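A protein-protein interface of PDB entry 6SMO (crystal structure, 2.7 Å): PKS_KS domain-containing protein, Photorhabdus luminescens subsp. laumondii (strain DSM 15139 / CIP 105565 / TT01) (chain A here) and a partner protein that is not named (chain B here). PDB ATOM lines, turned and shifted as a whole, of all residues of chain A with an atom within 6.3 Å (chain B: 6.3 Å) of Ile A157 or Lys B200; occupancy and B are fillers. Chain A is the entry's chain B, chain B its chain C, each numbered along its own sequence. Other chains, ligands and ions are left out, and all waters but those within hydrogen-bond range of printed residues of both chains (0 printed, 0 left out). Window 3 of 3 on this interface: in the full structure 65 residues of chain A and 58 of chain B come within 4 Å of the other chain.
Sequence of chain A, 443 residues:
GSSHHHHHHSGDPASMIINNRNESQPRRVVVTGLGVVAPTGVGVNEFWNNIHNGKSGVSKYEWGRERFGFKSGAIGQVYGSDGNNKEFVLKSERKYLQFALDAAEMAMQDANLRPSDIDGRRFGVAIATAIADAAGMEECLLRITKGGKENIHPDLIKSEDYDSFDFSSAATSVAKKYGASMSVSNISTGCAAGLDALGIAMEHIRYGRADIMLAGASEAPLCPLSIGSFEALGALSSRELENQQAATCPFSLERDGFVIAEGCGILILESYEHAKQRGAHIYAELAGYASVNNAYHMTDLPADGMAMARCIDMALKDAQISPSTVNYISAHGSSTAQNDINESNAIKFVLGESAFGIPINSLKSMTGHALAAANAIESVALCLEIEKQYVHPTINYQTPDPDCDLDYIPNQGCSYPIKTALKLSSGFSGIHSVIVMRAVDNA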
ATOM      1  N   CYS A 140      25.412 -16.778   6.799  1.00  0.00           N
ATOM      2  CA  CYS A 140      24.022 -16.242   6.815  1.00  0.00           C
ATOM      3  C   CYS A 140      24.037 -14.759   7.207  1.00  0.00           C
ATOM      4  O   CYS A 140      23.372 -13.965   6.519  1.00  0.00           O
ATOM      5  CB  CYS A 140      23.140 -17.029   7.777  1.00  0.00           C
ATOM      6  SG  CYS A 140      21.492 -16.310   8.007  1.00  0.00           S
ATOM      7  N   ARG A 143      25.714 -12.471   4.478  1.00  0.00           N
ATOM      8  CA  ARG A 143      24.859 -12.483   3.260  1.00  0.00           C
ATOM      9  C   ARG A 143      23.724 -11.462   3.423  1.00  0.00           C
ATOM     10  O   ARG A 143      23.511 -10.665   2.486  1.00  0.00           O
ATOM     11  CB  ARG A 143      24.303 -13.889   3.020  1.00  0.00           C
ATOM     12  CG  ARG A 143      23.501 -14.047   1.736  1.00  0.00           C
ATOM     13  CD  ARG A 143      22.356 -15.026   1.912  1.00  0.00           C
ATOM     14  NE  ARG A 143      22.802 -16.311   2.437  1.00  0.00           N
ATOM     15  CZ  ARG A 143      22.000 -17.260   2.917  1.00  0.00           C
ATOM     16  NH1 ARG A 143      22.517 -18.391   3.369  1.00  0.00           N
ATOM     17  NH2 ARG A 143      20.689 -17.082   2.948  1.00  0.00           N
ATOM     18  N   ILE A 144      23.031 -11.489   4.567  1.00  0.00           N
ATOM     19  CA  ILE A 144      21.824 -10.650   4.851  1.00  0.00           C
ATOM     20  C   ILE A 144      22.236  -9.188   5.091  1.00  0.00           C
ATOM     21  O   ILE A 144      21.361  -8.313   4.936  1.00  0.00           O
ATOM     22  CB  ILE A 144      20.996 -11.218   6.026  1.00  0.00           C
ATOM     23  CG1 ILE A 144      21.782 -11.255   7.342  1.00  0.00           C
ATOM     24  CG2 ILE A 144      20.426 -12.580   5.656  1.00  0.00           C
ATOM     25  CD1 ILE A 144      21.015 -11.825   8.518  1.00  0.00           C
ATOM     26  N   ILE A 152      20.881  -5.510   8.810  1.00  0.00           N
ATOM     27  CA  ILE A 152      20.278  -6.809   8.386  1.00  0.00           C
ATOM     28  C   ILE A 152      19.040  -6.529   7.525  1.00  0.00           C
ATOM     29  O   ILE A 152      18.151  -5.789   7.988  1.00  0.00           O
ATOM     30  CB  ILE A 152      19.950  -7.692   9.610  1.00  0.00           C
ATOM     31  CG1 ILE A 152      21.227  -8.242  10.253  1.00  0.00           C
ATOM     32  CG2 ILE A 152      18.983  -8.808   9.239  1.00  0.00           C
ATOM     33  CD1 ILE A 152      21.052  -8.699  11.679  1.00  0.00           C
ATOM     34  N   HIS A 153      19.003  -7.107   6.319  1.00  0.00           N
ATOM     35  CA  HIS A 153      17.848  -7.099   5.381  1.00  0.00           C
ATOM     36  C   HIS A 153      16.931  -8.275   5.713  1.00  0.00           C
ATOM     37  O   HIS A 153      17.324  -9.425   5.526  1.00  0.00           O
ATOM     38  CB  HIS A 153      18.335  -7.169   3.927  1.00  0.00           C
ATOM     39  CG  HIS A 153      18.991  -5.922   3.435  1.00  0.00           C
ATOM     40  ND1 HIS A 153      18.769  -5.425   2.166  1.00  0.00           N
ATOM     41  CD2 HIS A 153      19.852  -5.069   4.030  1.00  0.00           C
ATOM     42  CE1 HIS A 153      19.471  -4.323   1.998  1.00  0.00           C
ATOM     43  NE2 HIS A 153      20.144  -4.082   3.129  1.00  0.00           N
ATOM     44  N   PRO A 154      15.696  -8.041   6.219  1.00  0.00           N
ATOM     45  CA  PRO A 154      14.787  -9.138   6.563  1.00  0.00           C
ATOM     46  C   PRO A 154      14.431 -10.049   5.377  1.00  0.00           C
ATOM     47  O   PRO A 154      14.295 -11.242   5.588  1.00  0.00           O
ATOM     48  CB  PRO A 154      13.517  -8.430   7.066  1.00  0.00           C
ATOM     49  CG  PRO A 154      13.989  -7.049   7.473  1.00  0.00           C
ATOM     50  CD  PRO A 154      15.111  -6.722   6.510  1.00  0.00           C
ATOM     51  N   ASP A 155      14.292  -9.473   4.178  1.00  0.00           N
ATOM     52  CA  ASP A 155      13.825 -10.170   2.946  1.00  0.00           C
ATOM     53  C   ASP A 155      14.845 -11.231   2.506  1.00  0.00           C
ATOM     54  O   ASP A 155      14.406 -12.258   1.952  1.00  0.00           O
ATOM     55  CB  ASP A 155      13.534  -9.181   1.812  1.00  0.00           C
ATOM     56  CG  ASP A 155      14.726  -8.338   1.393  1.00  0.00           C
ATOM     57  OD1 ASP A 155      15.350  -7.727   2.282  1.00  0.00           O
ATOM     58  OD2 ASP A 155      15.022  -8.299   0.181  1.00  0.00           O
ATOM     59  N   LEU A 156      16.143 -11.000   2.740  1.00  0.00           N
ATOM     60  CA  LEU A 156      17.245 -11.888   2.267  1.00  0.00           C
ATOM     61  C   LEU A 156      17.351 -13.146   3.143  1.00  0.00           C
ATOM     62  O   LEU A 156      18.017 -14.102   2.695  1.00  0.00           O
ATOM     63  CB  LEU A 156      18.570 -11.117   2.257  1.00  0.00           C
ATOM     64  CG  LEU A 156      18.786 -10.168   1.076  1.00  0.00           C
ATOM     65  CD1 LEU A 156      20.060  -9.360   1.262  1.00  0.00           C
ATOM     66  CD2 LEU A 156      18.836 -10.925  -0.244  1.00  0.00           C
ATOM     67  N   ILE A 157      16.735 -13.157   4.332  1.00  0.00           N
ATOM     68  CA  ILE A 157      16.737 -14.332   5.258  1.00  0.00           C
ATOM     69  C   ILE A 157      15.898 -15.447   4.619  1.00  0.00           C
ATOM     70  O   ILE A 157      14.670 -15.269   4.502  1.00  0.00           O
ATOM     71  CB  ILE A 157      16.216 -13.964   6.664  1.00  0.00           C
ATOM     72  CG1 ILE A 157      17.059 -12.867   7.322  1.00  0.00           C
ATOM     73  CG2 ILE A 157      16.134 -15.202   7.548  1.00  0.00           C
ATOM     74  CD1 ILE A 157      16.371 -12.173   8.474  1.00  0.00           C
ATOM     75  N   LYS A 158      16.547 -16.550   4.232  1.00  0.00           N
ATOM     76  CA  LYS A 158      15.901 -17.731   3.596  1.00  0.00           C
ATOM     77  C   LYS A 158      15.314 -18.640   4.681  1.00  0.00           C
ATOM     78  O   LYS A 158      15.716 -18.506   5.854  1.00  0.00           O
ATOM     79  CB  LYS A 158      16.909 -18.496   2.731  1.00  0.00           C
ATOM     80  CG  LYS A 158      17.267 -17.826   1.412  1.00  0.00           C
ATOM     81  CD  LYS A 158      16.177 -17.933   0.367  1.00  0.00           C
ATOM     82  CE  LYS A 158      16.537 -17.254  -0.937  1.00  0.00           C
ATOM     83  NZ  LYS A 158      15.518 -17.506  -1.984  1.00  0.00           N
ATOM     84  N   SER A 159      14.396 -19.528   4.285  1.00  0.00           N
ATOM     85  CA  SER A 159      13.748 -20.549   5.152  1.00  0.00           C
ATOM     86  C   SER A 159      14.788 -21.574   5.625  1.00  0.00           C
ATOM     87  O   SER A 159      14.643 -22.083   6.755  1.00  0.00           O
ATOM     88  CB  SER A 159      12.607 -21.219   4.426  1.00  0.00           C
ATOM     89  OG  SER A 159      11.938 -22.143   5.270  1.00  0.00           O
ATOM     90  N   ASP A 161      17.937 -21.120   6.348  1.00  0.00           N
ATOM     91  CA  ASP A 161      18.964 -20.493   7.228  1.00  0.00           C
ATOM     92  C   ASP A 161      18.752 -20.888   8.697  1.00  0.00           C
ATOM     93  O   ASP A 161      19.751 -20.890   9.443  1.00  0.00           O
ATOM     94  CB  ASP A 161      18.961 -18.968   7.096  1.00  0.00           C
ATOM     95  CG  ASP A 161      19.525 -18.454   5.782  1.00  0.00           C
ATOM     96  OD1 ASP A 161      20.455 -19.093   5.249  1.00  0.00           O
ATOM     97  OD2 ASP A 161      19.032 -17.414   5.303  1.00  0.00           O
ATOM     98  N   SER B  43       5.328 -12.018  12.124  1.00  0.00           N
ATOM     99  CA  SER B  43       4.240 -11.390  12.926  1.00  0.00           C
ATOM    100  C   SER B  43       4.574 -11.444  14.424  1.00  0.00           C
ATOM    101  O   SER B  43       4.316 -10.440  15.118  1.00  0.00           O
ATOM    102  CB  SER B  43       2.910 -12.040  12.636  1.00  0.00           C
ATOM    103  OG  SER B  43       1.854 -11.352  13.290  1.00  0.00           O
ATOM    104  N   SER B  44       5.110 -12.575  14.900  1.00  0.00           N
ATOM    105  CA  SER B  44       5.583 -12.790  16.296  1.00  0.00           C
ATOM    106  C   SER B  44       6.670 -11.765  16.644  1.00  0.00           C
ATOM    107  O   SER B  44       7.416 -11.363  15.728  1.00  0.00           O
ATOM    108  CB  SER B  44       6.087 -14.199  16.485  1.00  0.00           C
ATOM    109  OG  SER B  44       5.101 -15.148  16.107  1.00  0.00           O
ATOM    110  N   LEU B 193      20.619 -10.464  14.727  1.00  0.00           N
ATOM    111  CA  LEU B 193      20.731 -11.667  13.854  1.00  0.00           C
ATOM    112  C   LEU B 193      19.603 -12.651  14.185  1.00  0.00           C
ATOM    113  O   LEU B 193      18.862 -13.026  13.253  1.00  0.00           O
ATOM    114  CB  LEU B 193      22.106 -12.322  14.032  1.00  0.00           C
ATOM    115  CG  LEU B 193      22.321 -13.633  13.270  1.00  0.00           C
ATOM    116  CD1 LEU B 193      22.018 -13.472  11.786  1.00  0.00           C
ATOM    117  CD2 LEU B 193      23.737 -14.150  13.467  1.00  0.00           C
ATOM    118  N   LYS B 195      17.047 -12.062  16.251  1.00  0.00           N
ATOM    119  CA  LYS B 195      15.776 -11.290  16.356  1.00  0.00           C
ATOM    120  C   LYS B 195      15.047 -11.336  15.007  1.00  0.00           C
ATOM    121  O   LYS B 195      13.863 -11.727  14.993  1.00  0.00           O
ATOM    122  CB  LYS B 195      16.034  -9.841  16.786  1.00  0.00           C
ATOM    123  CG  LYS B 195      14.788  -9.074  17.214  1.00  0.00           C
ATOM    124  CD  LYS B 195      15.075  -7.724  17.841  1.00  0.00           C
ATOM    125  CE  LYS B 195      15.218  -6.610  16.825  1.00  0.00           C
ATOM    126  NZ  LYS B 195      13.899  -6.123  16.354  1.00  0.00           N
ATOM    127  N   ASN B 196      15.736 -10.963  13.924  1.00  0.00           N
ATOM    128  CA  ASN B 196      15.191 -10.945  12.538  1.00  0.00           C
ATOM    129  C   ASN B 196      14.882 -12.377  12.081  1.00  0.00           C
ATOM    130  O   ASN B 196      13.934 -12.544  11.286  1.00  0.00           O
ATOM    131  CB  ASN B 196      16.143 -10.251  11.559  1.00  0.00           C
ATOM    132  CG  ASN B 196      16.169  -8.746  11.724  1.00  0.00           C
ATOM    133  OD1 ASN B 196      15.148  -8.082  11.563  1.00  0.00           O
ATOM    134  ND2 ASN B 196      17.334  -8.199  12.030  1.00  0.00           N
ATOM    135  N   LEU B 197      15.649 -13.363  12.560  1.00  0.00           N
ATOM    136  CA  LEU B 197      15.487 -14.801  12.210  1.00  0.00           C
ATOM    137  C   LEU B 197      14.154 -15.318  12.766  1.00  0.00           C
ATOM    138  O   LEU B 197      13.369 -15.881  11.979  1.00  0.00           O
ATOM    139  CB  LEU B 197      16.666 -15.600  12.777  1.00  0.00           C
ATOM    140  CG  LEU B 197      16.745 -17.061  12.331  1.00  0.00           C
ATOM    141  CD1 LEU B 197      17.296 -17.168  10.917  1.00  0.00           C
ATOM    142  CD2 LEU B 197      17.590 -17.881  13.294  1.00  0.00           C
ATOM    143  N   LEU B 198      13.915 -15.130  14.069  1.00  0.00           N
ATOM    144  CA  LEU B 198      12.724 -15.656  14.794  1.00  0.00           C
ATOM    145  C   LEU B 198      11.453 -14.930  14.334  1.00  0.00           C
ATOM    146  O   LEU B 198      10.384 -15.571  14.331  1.00  0.00           O
ATOM    147  CB  LEU B 198      12.925 -15.491  16.306  1.00  0.00           C
ATOM    148  CG  LEU B 198      14.027 -16.343  16.937  1.00  0.00           C
ATOM    149  CD1 LEU B 198      14.087 -16.114  18.439  1.00  0.00           C
ATOM    150  CD2 LEU B 198      13.831 -17.821  16.636  1.00  0.00           C
ATOM    151  N   GLU B 199      11.561 -13.648  13.969  1.00  0.00           N
ATOM    152  CA  GLU B 199      10.408 -12.794  13.566  1.00  0.00           C
ATOM    153  C   GLU B 199       9.856 -13.244  12.205  1.00  0.00           C
ATOM    154  O   GLU B 199       8.665 -12.981  11.952  1.00  0.00           O
ATOM    155  CB  GLU B 199      10.809 -11.318  13.529  1.00  0.00           C
ATOM    156  CG  GLU B 199      10.824 -10.665  14.900  1.00  0.00           C
ATOM    157  CD  GLU B 199      11.208  -9.195  14.911  1.00  0.00           C
ATOM    158  OE1 GLU B 199      10.714  -8.464  15.792  1.00  0.00           O
ATOM    159  OE2 GLU B 199      12.005  -8.784  14.044  1.00  0.00           O
ATOM    160  N   LYS B 200      10.678 -13.890  11.367  1.00  0.00           N
ATOM    161  CA  LYS B 200      10.305 -14.298   9.984  1.00  0.00           C
ATOM    162  C   LYS B 200      10.082 -15.816   9.915  1.00  0.00           C
ATOM    163  O   LYS B 200       8.919 -16.228   9.740  1.00  0.00           O
ATOM    164  CB  LYS B 200      11.379 -13.849   8.988  1.00  0.00           C
ATOM    165  CG  LYS B 200      10.960 -13.915   7.525  1.00  0.00           C
ATOM    166  CD  LYS B 200      12.056 -13.528   6.555  1.00  0.00           C
ATOM    167  CE  LYS B 200      11.597 -13.524   5.111  1.00  0.00           C
ATOM    168  NZ  LYS B 200      11.325 -14.894   4.613  1.00  0.00           N
ATOM    169  N   THR B 201      11.152 -16.609  10.053  1.00  0.00           N
ATOM    170  CA  THR B 201      11.213 -18.047   9.660  1.00  0.00           C
ATOM    171  C   THR B 201      10.411 -18.926  10.630  1.00  0.00           C
ATOM    172  O   THR B 201       9.699 -19.827  10.138  1.00  0.00           O
ATOM    173  CB  THR B 201      12.665 -18.534   9.560  1.00  0.00           C
ATOM    174  OG1 THR B 201      13.327 -18.240  10.790  1.00  0.00           O
ATOM    175  CG2 THR B 201      13.417 -17.903   8.407  1.00  0.00           C
ATOM    176  N   SER B 202      10.523 -18.684  11.942  1.00  0.00           N
ATOM    177  CA  SER B 202      10.000 -19.563  13.025  1.00  0.00           C
ATOM    178  C   SER B 202       8.473 -19.708  12.940  1.00  0.00           C
ATOM    179  O   SER B 202       7.971 -20.792  13.300  1.00  0.00           O
ATOM    180  CB  SER B 202      10.423 -19.063  14.382  1.00  0.00           C
ATOM    181  OG  SER B 202      11.832 -19.151  14.535  1.00  0.00           O
ATOM    182  N   SER B 203       7.768 -18.664  12.488  1.00  0.00           N
ATOM    183  CA  SER B 203       6.283 -18.601  12.409  1.00  0.00           C
ATOM    184  C   SER B 203       5.749 -19.652  11.426  1.00  0.00           C
ATOM    185  O   SER B 203       4.822 -20.395  11.809  1.00  0.00           O
ATOM    186  CB  SER B 203       5.821 -17.217  12.031  1.00  0.00           C
ATOM    187  OG  SER B 203       6.252 -16.260  12.988  1.00  0.00           O
ATOM    188  N   GLN B 204       6.313 -19.711  10.214  1.00  0.00           N
ATOM    189  CA  GLN B 204       5.808 -20.543   9.085  1.00  0.00           C
ATOM    190  C   GLN B 204       6.233 -22.009   9.251  1.00  0.00           C
ATOM    191  O   GLN B 204       5.489 -22.884   8.765  1.00  0.00           O
ATOM    192  CB  GLN B 204       6.309 -20.004   7.741  1.00  0.00           C
ATOM    193  CG  GLN B 204       5.709 -18.657   7.353  1.00  0.00           C
ATOM    194  CD  GLN B 204       6.598 -17.491   7.713  1.00  0.00           C
ATOM    195  OE1 GLN B 204       7.766 -17.435   7.331  1.00  0.00           O
ATOM    196  NE2 GLN B 204       6.044 -16.536   8.443  1.00  0.00           N
ATOM    197  N   LYS B 205       7.378 -22.269   9.892  1.00  0.00           N
ATOM    198  CA  LYS B 205       7.981 -23.627  10.007  1.00  0.00           C
ATOM    199  C   LYS B 205       7.083 -24.536  10.854  1.00  0.00           C
ATOM    200  O   LYS B 205       6.754 -24.149  11.994  1.00  0.00           O
ATOM    201  CB  LYS B 205       9.390 -23.562  10.608  1.00  0.00           C
ATOM    202  CG  LYS B 205      10.506 -23.327   9.599  1.00  0.00           C
ATOM    203  CD  LYS B 205      11.885 -23.670  10.122  1.00  0.00           C
ATOM    204  CE  LYS B 205      12.902 -23.876   9.019  1.00  0.00           C
ATOM    205  NZ  LYS B 205      12.720 -25.179   8.336  1.00  0.00           N
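N of His A153 is in hydrogen-bond range of O of Ile A144 (3.0 Å). The backbone NH (N) of Lys A158 is in hydrogen-bond range of the side-chain carboxylate (OD2) of Asp A161. The backbone carbonyl oxygen of Leu B197 sits at hydrogen-bond distance from the side-chain hydroxyl of Thr B201 (2.6 Å). The backbone carbonyl oxygen of Lys B200 sits close to the side-chain amide oxygen of Gln B204 (2.9 Å).
Of the 14 printed residues of chain B, 5 touch a printed residue of chain A. Hydrophobic or aromatic side chains of chain B within 4 Å of the printed part of chain A: Leu B193. Of the 12 printed residues of chain A, 6 touch a printed residue of chain B. Printed residues of chain A that touch a printed residue of chain B: Ile A144, Ile A152, Pro A154, Ile A157, Lys A158 and Ser A159. Hydrophobic or aromatic side chains of chain A within 4 Å of the printed part of chain B: Ile A144, Ile A152 and Ile A157. Among the printed residues, 9 pairs touch across the chains. Among the printed residues, no Asp or Glu carboxylate lies within 4 Å of a Lys or Arg side-chain nitrogen of the other chain.
Among the printed residues, pairs that only touch across the chains: Ile A152 with Asn B196 (3.3 Å), Pro A154 with Lys B200 (3.3 Å), Ser A159 with Lys B205 (3.4 Å), Lys A158 with Thr B201 (3.5 Å), Ile A152 with Leu B193 (3.5 Å), Ile A157 with Asn B196 (3.6 Å), Ile A144 with Leu B193 (3.8 Å) and Ile A157 with Thr B201 (3.9 Å).
Printed residues of chain B within 4 Å of Ile A144: Leu B193. Printed residues of chain B within 4 Å of Ile A152: Leu B193 (3.5 Å) and Asn B196 (3.3 Å). Printed residues of chain B within 4 Å of Ile A157: Asn B196, Lys B200 and Thr B201. Of the printed residues of chain B, Lys A158 touches Thr B201 (3.5 Å). Ser B44 touches none of the printed residues of chain A. Of the printed residues of chain A, Asn B196 touches Ile A152 (3.3 Å) and Ile A157 (3.6 Å). Of the printed residues of chain A, Lys B200 touches Pro A154 and Ile A157. Of the printed residues of chain A, Thr B201 touches Ile A157 (3.9 Å) and Lys A158 (3.5 Å). The nearest residue of chain B that does not touch Ile A157 is Leu B197 (4.1 Å).
The backbone carbonyl oxygen of Ile A157 lies within hydrogen-bond range of the side-chain amino group of Lys B200 (3.4 Å).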
